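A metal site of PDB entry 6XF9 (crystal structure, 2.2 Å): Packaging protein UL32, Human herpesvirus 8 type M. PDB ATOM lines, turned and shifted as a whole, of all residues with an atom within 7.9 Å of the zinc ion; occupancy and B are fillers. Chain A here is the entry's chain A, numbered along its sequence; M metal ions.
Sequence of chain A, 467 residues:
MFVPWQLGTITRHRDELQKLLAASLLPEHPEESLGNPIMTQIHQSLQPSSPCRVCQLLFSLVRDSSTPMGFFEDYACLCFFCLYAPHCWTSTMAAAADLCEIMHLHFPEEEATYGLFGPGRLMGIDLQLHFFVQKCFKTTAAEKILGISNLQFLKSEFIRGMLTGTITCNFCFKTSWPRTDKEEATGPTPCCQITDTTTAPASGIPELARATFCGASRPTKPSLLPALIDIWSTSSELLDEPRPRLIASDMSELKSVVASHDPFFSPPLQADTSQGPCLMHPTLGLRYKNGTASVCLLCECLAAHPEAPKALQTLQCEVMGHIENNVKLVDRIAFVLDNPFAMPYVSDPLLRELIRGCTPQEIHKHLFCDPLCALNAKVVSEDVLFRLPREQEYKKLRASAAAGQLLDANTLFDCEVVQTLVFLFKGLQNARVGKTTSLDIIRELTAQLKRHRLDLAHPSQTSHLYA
O of Gln 448 lies within hydrogen-bond range of ND1 of His 452, 2.7 Å away. The side-chain sulfur of Cys 191 lies close to the side-chain hydroxyl of Thr 195. The side-chain sulfur (SG) of Cys 191 lies close to the guanidinium group (NH2) of Arg 451 (3.8 Å). N of Val 418 lies close to SG of Cys 415, at 3.7 Å. N of Val 417 lies close to SG of Cys 415 (3.7 Å). The side-chain sulfur of Cys 192 sits close to the backbone NH of Ile 194, 3.7 Å away.
The nearest printed residue that does not touch the zinc ion is Thr 195 (4.2 Å).
The zinc ion is bound by a ring nitrogen (NE2) of His 452 (2.0 Å), the side-chain sulfur of Cys 191 (2.3 Å), the side-chain sulfur of Cys 415 (2.3 Å) and the side-chain sulfur of Cys 192 (2.4 Å).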
ATOM      1  N   PRO A 190     -18.849  -1.165 -24.666  1.00  0.00           N
ATOM      2  CA  PRO A 190     -20.164  -1.784 -24.827  1.00  0.00           C
ATOM      3  C   PRO A 190     -20.846  -1.963 -23.487  1.00  0.00           C
ATOM      4  O   PRO A 190     -20.212  -1.972 -22.439  1.00  0.00           O
ATOM      5  CB  PRO A 190     -19.847  -3.141 -25.488  1.00  0.00           C
ATOM      6  CG  PRO A 190     -18.568  -2.908 -26.178  1.00  0.00           C
ATOM      7  CD  PRO A 190     -17.790  -1.997 -25.269  1.00  0.00           C
ATOM      8  N   CYS A 191     -22.185  -1.952 -23.518  1.00  0.00           N
ATOM      9  CA  CYS A 191     -22.933  -2.019 -22.266  1.00  0.00           C
ATOM     10  C   CYS A 191     -22.825  -3.385 -21.615  1.00  0.00           C
ATOM     11  O   CYS A 191     -22.773  -3.495 -20.387  1.00  0.00           O
ATOM     12  CB  CYS A 191     -24.398  -1.631 -22.502  1.00  0.00           C
ATOM     13  SG  CYS A 191     -25.108  -2.410 -23.922  1.00  0.00           S
ATOM     14  N   CYS A 192     -22.748  -4.447 -22.425  1.00  0.00           N
ATOM     15  CA  CYS A 192     -22.775  -5.813 -21.889  1.00  0.00           C
ATOM     16  C   CYS A 192     -22.003  -6.718 -22.845  1.00  0.00           C
ATOM     17  O   CYS A 192     -21.231  -6.248 -23.691  1.00  0.00           O
ATOM     18  CB  CYS A 192     -24.219  -6.271 -21.691  1.00  0.00           C
ATOM     19  SG  CYS A 192     -25.229  -6.272 -23.200  1.00  0.00           S
ATOM     20  N   GLN A 193     -22.195  -8.031 -22.715  1.00  0.00           N
ATOM     21  CA  GLN A 193     -21.453  -8.950 -23.559  1.00  0.00           C
ATOM     22  C   GLN A 193     -22.160  -9.193 -24.883  1.00  0.00           C
ATOM     23  O   GLN A 193     -21.492  -9.514 -25.886  1.00  0.00           O
ATOM     24  CB  GLN A 193     -21.230 -10.265 -22.834  1.00  0.00           C
ATOM     25  CG  GLN A 193     -20.255 -10.093 -21.676  1.00  0.00           C
ATOM     26  CD  GLN A 193     -18.828 -10.395 -22.089  1.00  0.00           C
ATOM     27  OE1 GLN A 193     -18.601 -11.136 -23.050  1.00  0.00           O
ATOM     28  NE2 GLN A 193     -17.842  -9.828 -21.356  1.00  0.00           N
ATOM     29  N   ILE A 194     -23.480  -9.050 -24.933  1.00  0.00           N
ATOM     30  CA  ILE A 194     -24.191  -9.223 -26.195  1.00  0.00           C
ATOM     31  C   ILE A 194     -23.716  -8.198 -27.211  1.00  0.00           C
ATOM     32  O   ILE A 194     -23.608  -8.497 -28.404  1.00  0.00           O
ATOM     33  CB  ILE A 194     -25.707  -9.127 -25.980  1.00  0.00           C
ATOM     34  CG1 ILE A 194     -26.164 -10.210 -25.015  1.00  0.00           C
ATOM     35  CG2 ILE A 194     -26.436  -9.197 -27.313  1.00  0.00           C
ATOM     36  CD1 ILE A 194     -27.638 -10.130 -24.749  1.00  0.00           C
ATOM     37  N   THR A 195     -23.428  -6.972 -26.756  1.00  0.00           N
ATOM     38  CA  THR A 195     -22.994  -5.932 -27.673  1.00  0.00           C
ATOM     39  C   THR A 195     -21.507  -5.739 -27.686  1.00  0.00           C
ATOM     40  O   THR A 195     -21.012  -4.925 -28.473  1.00  0.00           O
ATOM     41  CB  THR A 195     -23.675  -4.602 -27.356  1.00  0.00           C
ATOM     42  OG1 THR A 195     -23.309  -4.158 -26.047  1.00  0.00           O
ATOM     43  CG2 THR A 195     -25.180  -4.743 -27.507  1.00  0.00           C
ATOM     44  N   ASP A 196     -20.758  -6.442 -26.838  1.00  0.00           N
ATOM     45  CA  ASP A 196     -19.309  -6.458 -26.940  1.00  0.00           C
ATOM     46  C   ASP A 196     -18.922  -7.572 -27.905  1.00  0.00           C
ATOM     47  O   ASP A 196     -18.948  -8.754 -27.552  1.00  0.00           O
ATOM     48  CB  ASP A 196     -18.642  -6.633 -25.582  1.00  0.00           C
ATOM     49  CG  ASP A 196     -17.160  -6.435 -25.660  1.00  0.00           C
ATOM     50  OD1 ASP A 196     -16.627  -6.576 -26.795  1.00  0.00           O
ATOM     51  OD2 ASP A 196     -16.517  -6.109 -24.620  1.00  0.00           O
ATOM     52  N   PHE A 413     -27.454 -13.427 -19.265  1.00  0.00           N
ATOM     53  CA  PHE A 413     -27.790 -12.070 -19.647  1.00  0.00           C
ATOM     54  C   PHE A 413     -27.538 -11.108 -18.519  1.00  0.00           C
ATOM     55  O   PHE A 413     -28.088 -11.264 -17.517  1.00  0.00           O
ATOM     56  CB  PHE A 413     -29.242 -11.977 -20.030  1.00  0.00           C
ATOM     57  CG  PHE A 413     -29.607 -10.667 -20.604  1.00  0.00           C
ATOM     58  CD1 PHE A 413     -29.862  -9.623 -19.813  1.00  0.00           C
ATOM     59  CD2 PHE A 413     -29.675 -10.494 -21.948  1.00  0.00           C
ATOM     60  CE1 PHE A 413     -30.168  -8.409 -20.338  1.00  0.00           C
ATOM     61  CE2 PHE A 413     -29.989  -9.291 -22.477  1.00  0.00           C
ATOM     62  CZ  PHE A 413     -30.238  -8.245 -21.678  1.00  0.00           C
ATOM     63  N   ASP A 414     -26.788 -10.040 -18.724  1.00  0.00           N
ATOM     64  CA  ASP A 414     -26.546  -9.051 -17.663  1.00  0.00           C
ATOM     65  C   ASP A 414     -26.276  -7.697 -18.309  1.00  0.00           C
ATOM     66  O   ASP A 414     -25.267  -7.541 -19.000  1.00  0.00           O
ATOM     67  CB  ASP A 414     -25.360  -9.480 -16.792  1.00  0.00           C
ATOM     68  CG  ASP A 414     -25.234  -8.626 -15.519  1.00  0.00           C
ATOM     69  OD1 ASP A 414     -25.462  -7.403 -15.598  1.00  0.00           O
ATOM     70  OD2 ASP A 414     -24.860  -9.152 -14.446  1.00  0.00           O
ATOM     71  N   CYS A 415     -27.186  -6.735 -18.123  1.00  0.00           N
ATOM     72  CA  CYS A 415     -26.986  -5.404 -18.688  1.00  0.00           C
ATOM     73  C   CYS A 415     -27.761  -4.379 -17.863  1.00  0.00           C
ATOM     74  O   CYS A 415     -28.998  -4.391 -17.867  1.00  0.00           O
ATOM     75  CB  CYS A 415     -27.435  -5.352 -20.141  1.00  0.00           C
ATOM     76  SG  CYS A 415     -26.914  -3.766 -20.888  1.00  0.00           S
ATOM     77  N   GLU A 416     -27.033  -3.511 -17.142  1.00  0.00           N
ATOM     78  CA  GLU A 416     -27.713  -2.498 -16.341  1.00  0.00           C
ATOM     79  C   GLU A 416     -28.385  -1.440 -17.207  1.00  0.00           C
ATOM     80  O   GLU A 416     -29.336  -0.774 -16.753  1.00  0.00           O
ATOM     81  CB  GLU A 416     -26.736  -1.856 -15.338  1.00  0.00           C
ATOM     82  CG  GLU A 416     -27.467  -1.261 -14.099  1.00  0.00           C
ATOM     83  CD  GLU A 416     -26.565  -1.058 -12.862  1.00  0.00           C
ATOM     84  OE1 GLU A 416     -27.106  -0.898 -11.713  1.00  0.00           O
ATOM     85  OE2 GLU A 416     -25.316  -1.099 -13.028  1.00  0.00           O
ATOM     86  N   VAL A 417     -27.908  -1.221 -18.438  1.00  0.00           N
ATOM     87  CA  VAL A 417     -28.582  -0.309 -19.364  1.00  0.00           C
ATOM     88  C   VAL A 417     -29.980  -0.820 -19.706  1.00  0.00           C
ATOM     89  O   VAL A 417     -30.962  -0.096 -19.584  1.00  0.00           O
ATOM     90  CB  VAL A 417     -27.742  -0.073 -20.628  1.00  0.00           C
ATOM     91  CG1 VAL A 417     -28.589   0.631 -21.704  1.00  0.00           C
ATOM     92  CG2 VAL A 417     -26.537   0.762 -20.279  1.00  0.00           C
ATOM     93  N   VAL A 418     -30.074  -2.050 -20.217  1.00  0.00           N
ATOM     94  CA  VAL A 418     -31.405  -2.606 -20.492  1.00  0.00           C
ATOM     95  C   VAL A 418     -32.203  -2.807 -19.209  1.00  0.00           C
ATOM     96  O   VAL A 418     -33.421  -2.573 -19.172  1.00  0.00           O
ATOM     97  CB  VAL A 418     -31.307  -3.905 -21.311  1.00  0.00           C
ATOM     98  CG1 VAL A 418     -32.638  -4.657 -21.251  1.00  0.00           C
ATOM     99  CG2 VAL A 418     -31.003  -3.551 -22.736  1.00  0.00           C
ATOM    100  N   GLN A 419     -31.560  -3.240 -18.126  1.00  0.00           N
ATOM    101  CA  GLN A 419     -32.326  -3.402 -16.896  1.00  0.00           C
ATOM    102  C   GLN A 419     -33.006  -2.085 -16.533  1.00  0.00           C
ATOM    103  O   GLN A 419     -34.223  -2.045 -16.286  1.00  0.00           O
ATOM    104  CB  GLN A 419     -31.437  -3.884 -15.751  1.00  0.00           C
ATOM    105  CG  GLN A 419     -32.203  -4.306 -14.490  1.00  0.00           C
ATOM    106  CD  GLN A 419     -31.405  -4.125 -13.184  1.00  0.00           C
ATOM    107  OE1 GLN A 419     -30.455  -3.341 -13.102  1.00  0.00           O
ATOM    108  NE2 GLN A 419     -31.769  -4.891 -12.171  1.00  0.00           N
ATOM    109  N   GLN A 448     -32.677  -0.390 -27.720  1.00  0.00           N
ATOM    110  CA  GLN A 448     -31.843  -1.330 -26.991  1.00  0.00           C
ATOM    111  C   GLN A 448     -32.358  -2.762 -27.128  1.00  0.00           C
ATOM    112  O   GLN A 448     -31.570  -3.714 -27.199  1.00  0.00           O
ATOM    113  CB  GLN A 448     -31.791  -0.906 -25.542  1.00  0.00           C
ATOM    114  CG  GLN A 448     -31.260   0.506 -25.371  1.00  0.00           C
ATOM    115  CD  GLN A 448     -29.755   0.581 -25.524  1.00  0.00           C
ATOM    116  OE1 GLN A 448     -29.113  -0.428 -25.818  1.00  0.00           O
ATOM    117  NE2 GLN A 448     -29.185   1.755 -25.282  1.00  0.00           N
ATOM    118  N   ARG A 451     -30.881  -3.825 -30.423  1.00  0.00           N
ATOM    119  CA  ARG A 451     -29.438  -4.032 -30.309  1.00  0.00           C
ATOM    120  C   ARG A 451     -29.109  -5.318 -29.562  1.00  0.00           C
ATOM    121  O   ARG A 451     -28.015  -5.857 -29.732  1.00  0.00           O
ATOM    122  CB  ARG A 451     -28.761  -2.899 -29.548  1.00  0.00           C
ATOM    123  CG  ARG A 451     -28.310  -1.727 -30.359  1.00  0.00           C
ATOM    124  CD  ARG A 451     -27.822  -0.721 -29.366  1.00  0.00           C
ATOM    125  NE  ARG A 451     -26.458  -0.984 -28.947  1.00  0.00           N
ATOM    126  CZ  ARG A 451     -26.009  -0.727 -27.718  1.00  0.00           C
ATOM    127  NH1 ARG A 451     -26.852  -0.245 -26.821  1.00  0.00           N
ATOM    128  NH2 ARG A 451     -24.730  -0.957 -27.400  1.00  0.00           N
ATOM    129  N   HIS A 452     -29.990  -5.775 -28.694  1.00  0.00           N
ATOM    130  CA  HIS A 452     -29.748  -6.970 -27.888  1.00  0.00           C
ATOM    131  C   HIS A 452     -30.454  -8.202 -28.429  1.00  0.00           C
ATOM    132  O   HIS A 452     -30.499  -9.227 -27.743  1.00  0.00           O
ATOM    133  CB  HIS A 452     -30.157  -6.708 -26.437  1.00  0.00           C
ATOM    134  CG  HIS A 452     -29.251  -5.754 -25.721  1.00  0.00           C
ATOM    135  ND1 HIS A 452     -29.398  -4.385 -25.794  1.00  0.00           N
ATOM    136  CD2 HIS A 452     -28.168  -5.962 -24.927  1.00  0.00           C
ATOM    137  CE1 HIS A 452     -28.461  -3.802 -25.064  1.00  0.00           C
ATOM    138  NE2 HIS A 452     -27.685  -4.738 -24.545  1.00  0.00           N
HETATM  139 ZN    ZN M   1     -26.352  -4.205 -23.108  1.00  0.00          ZN
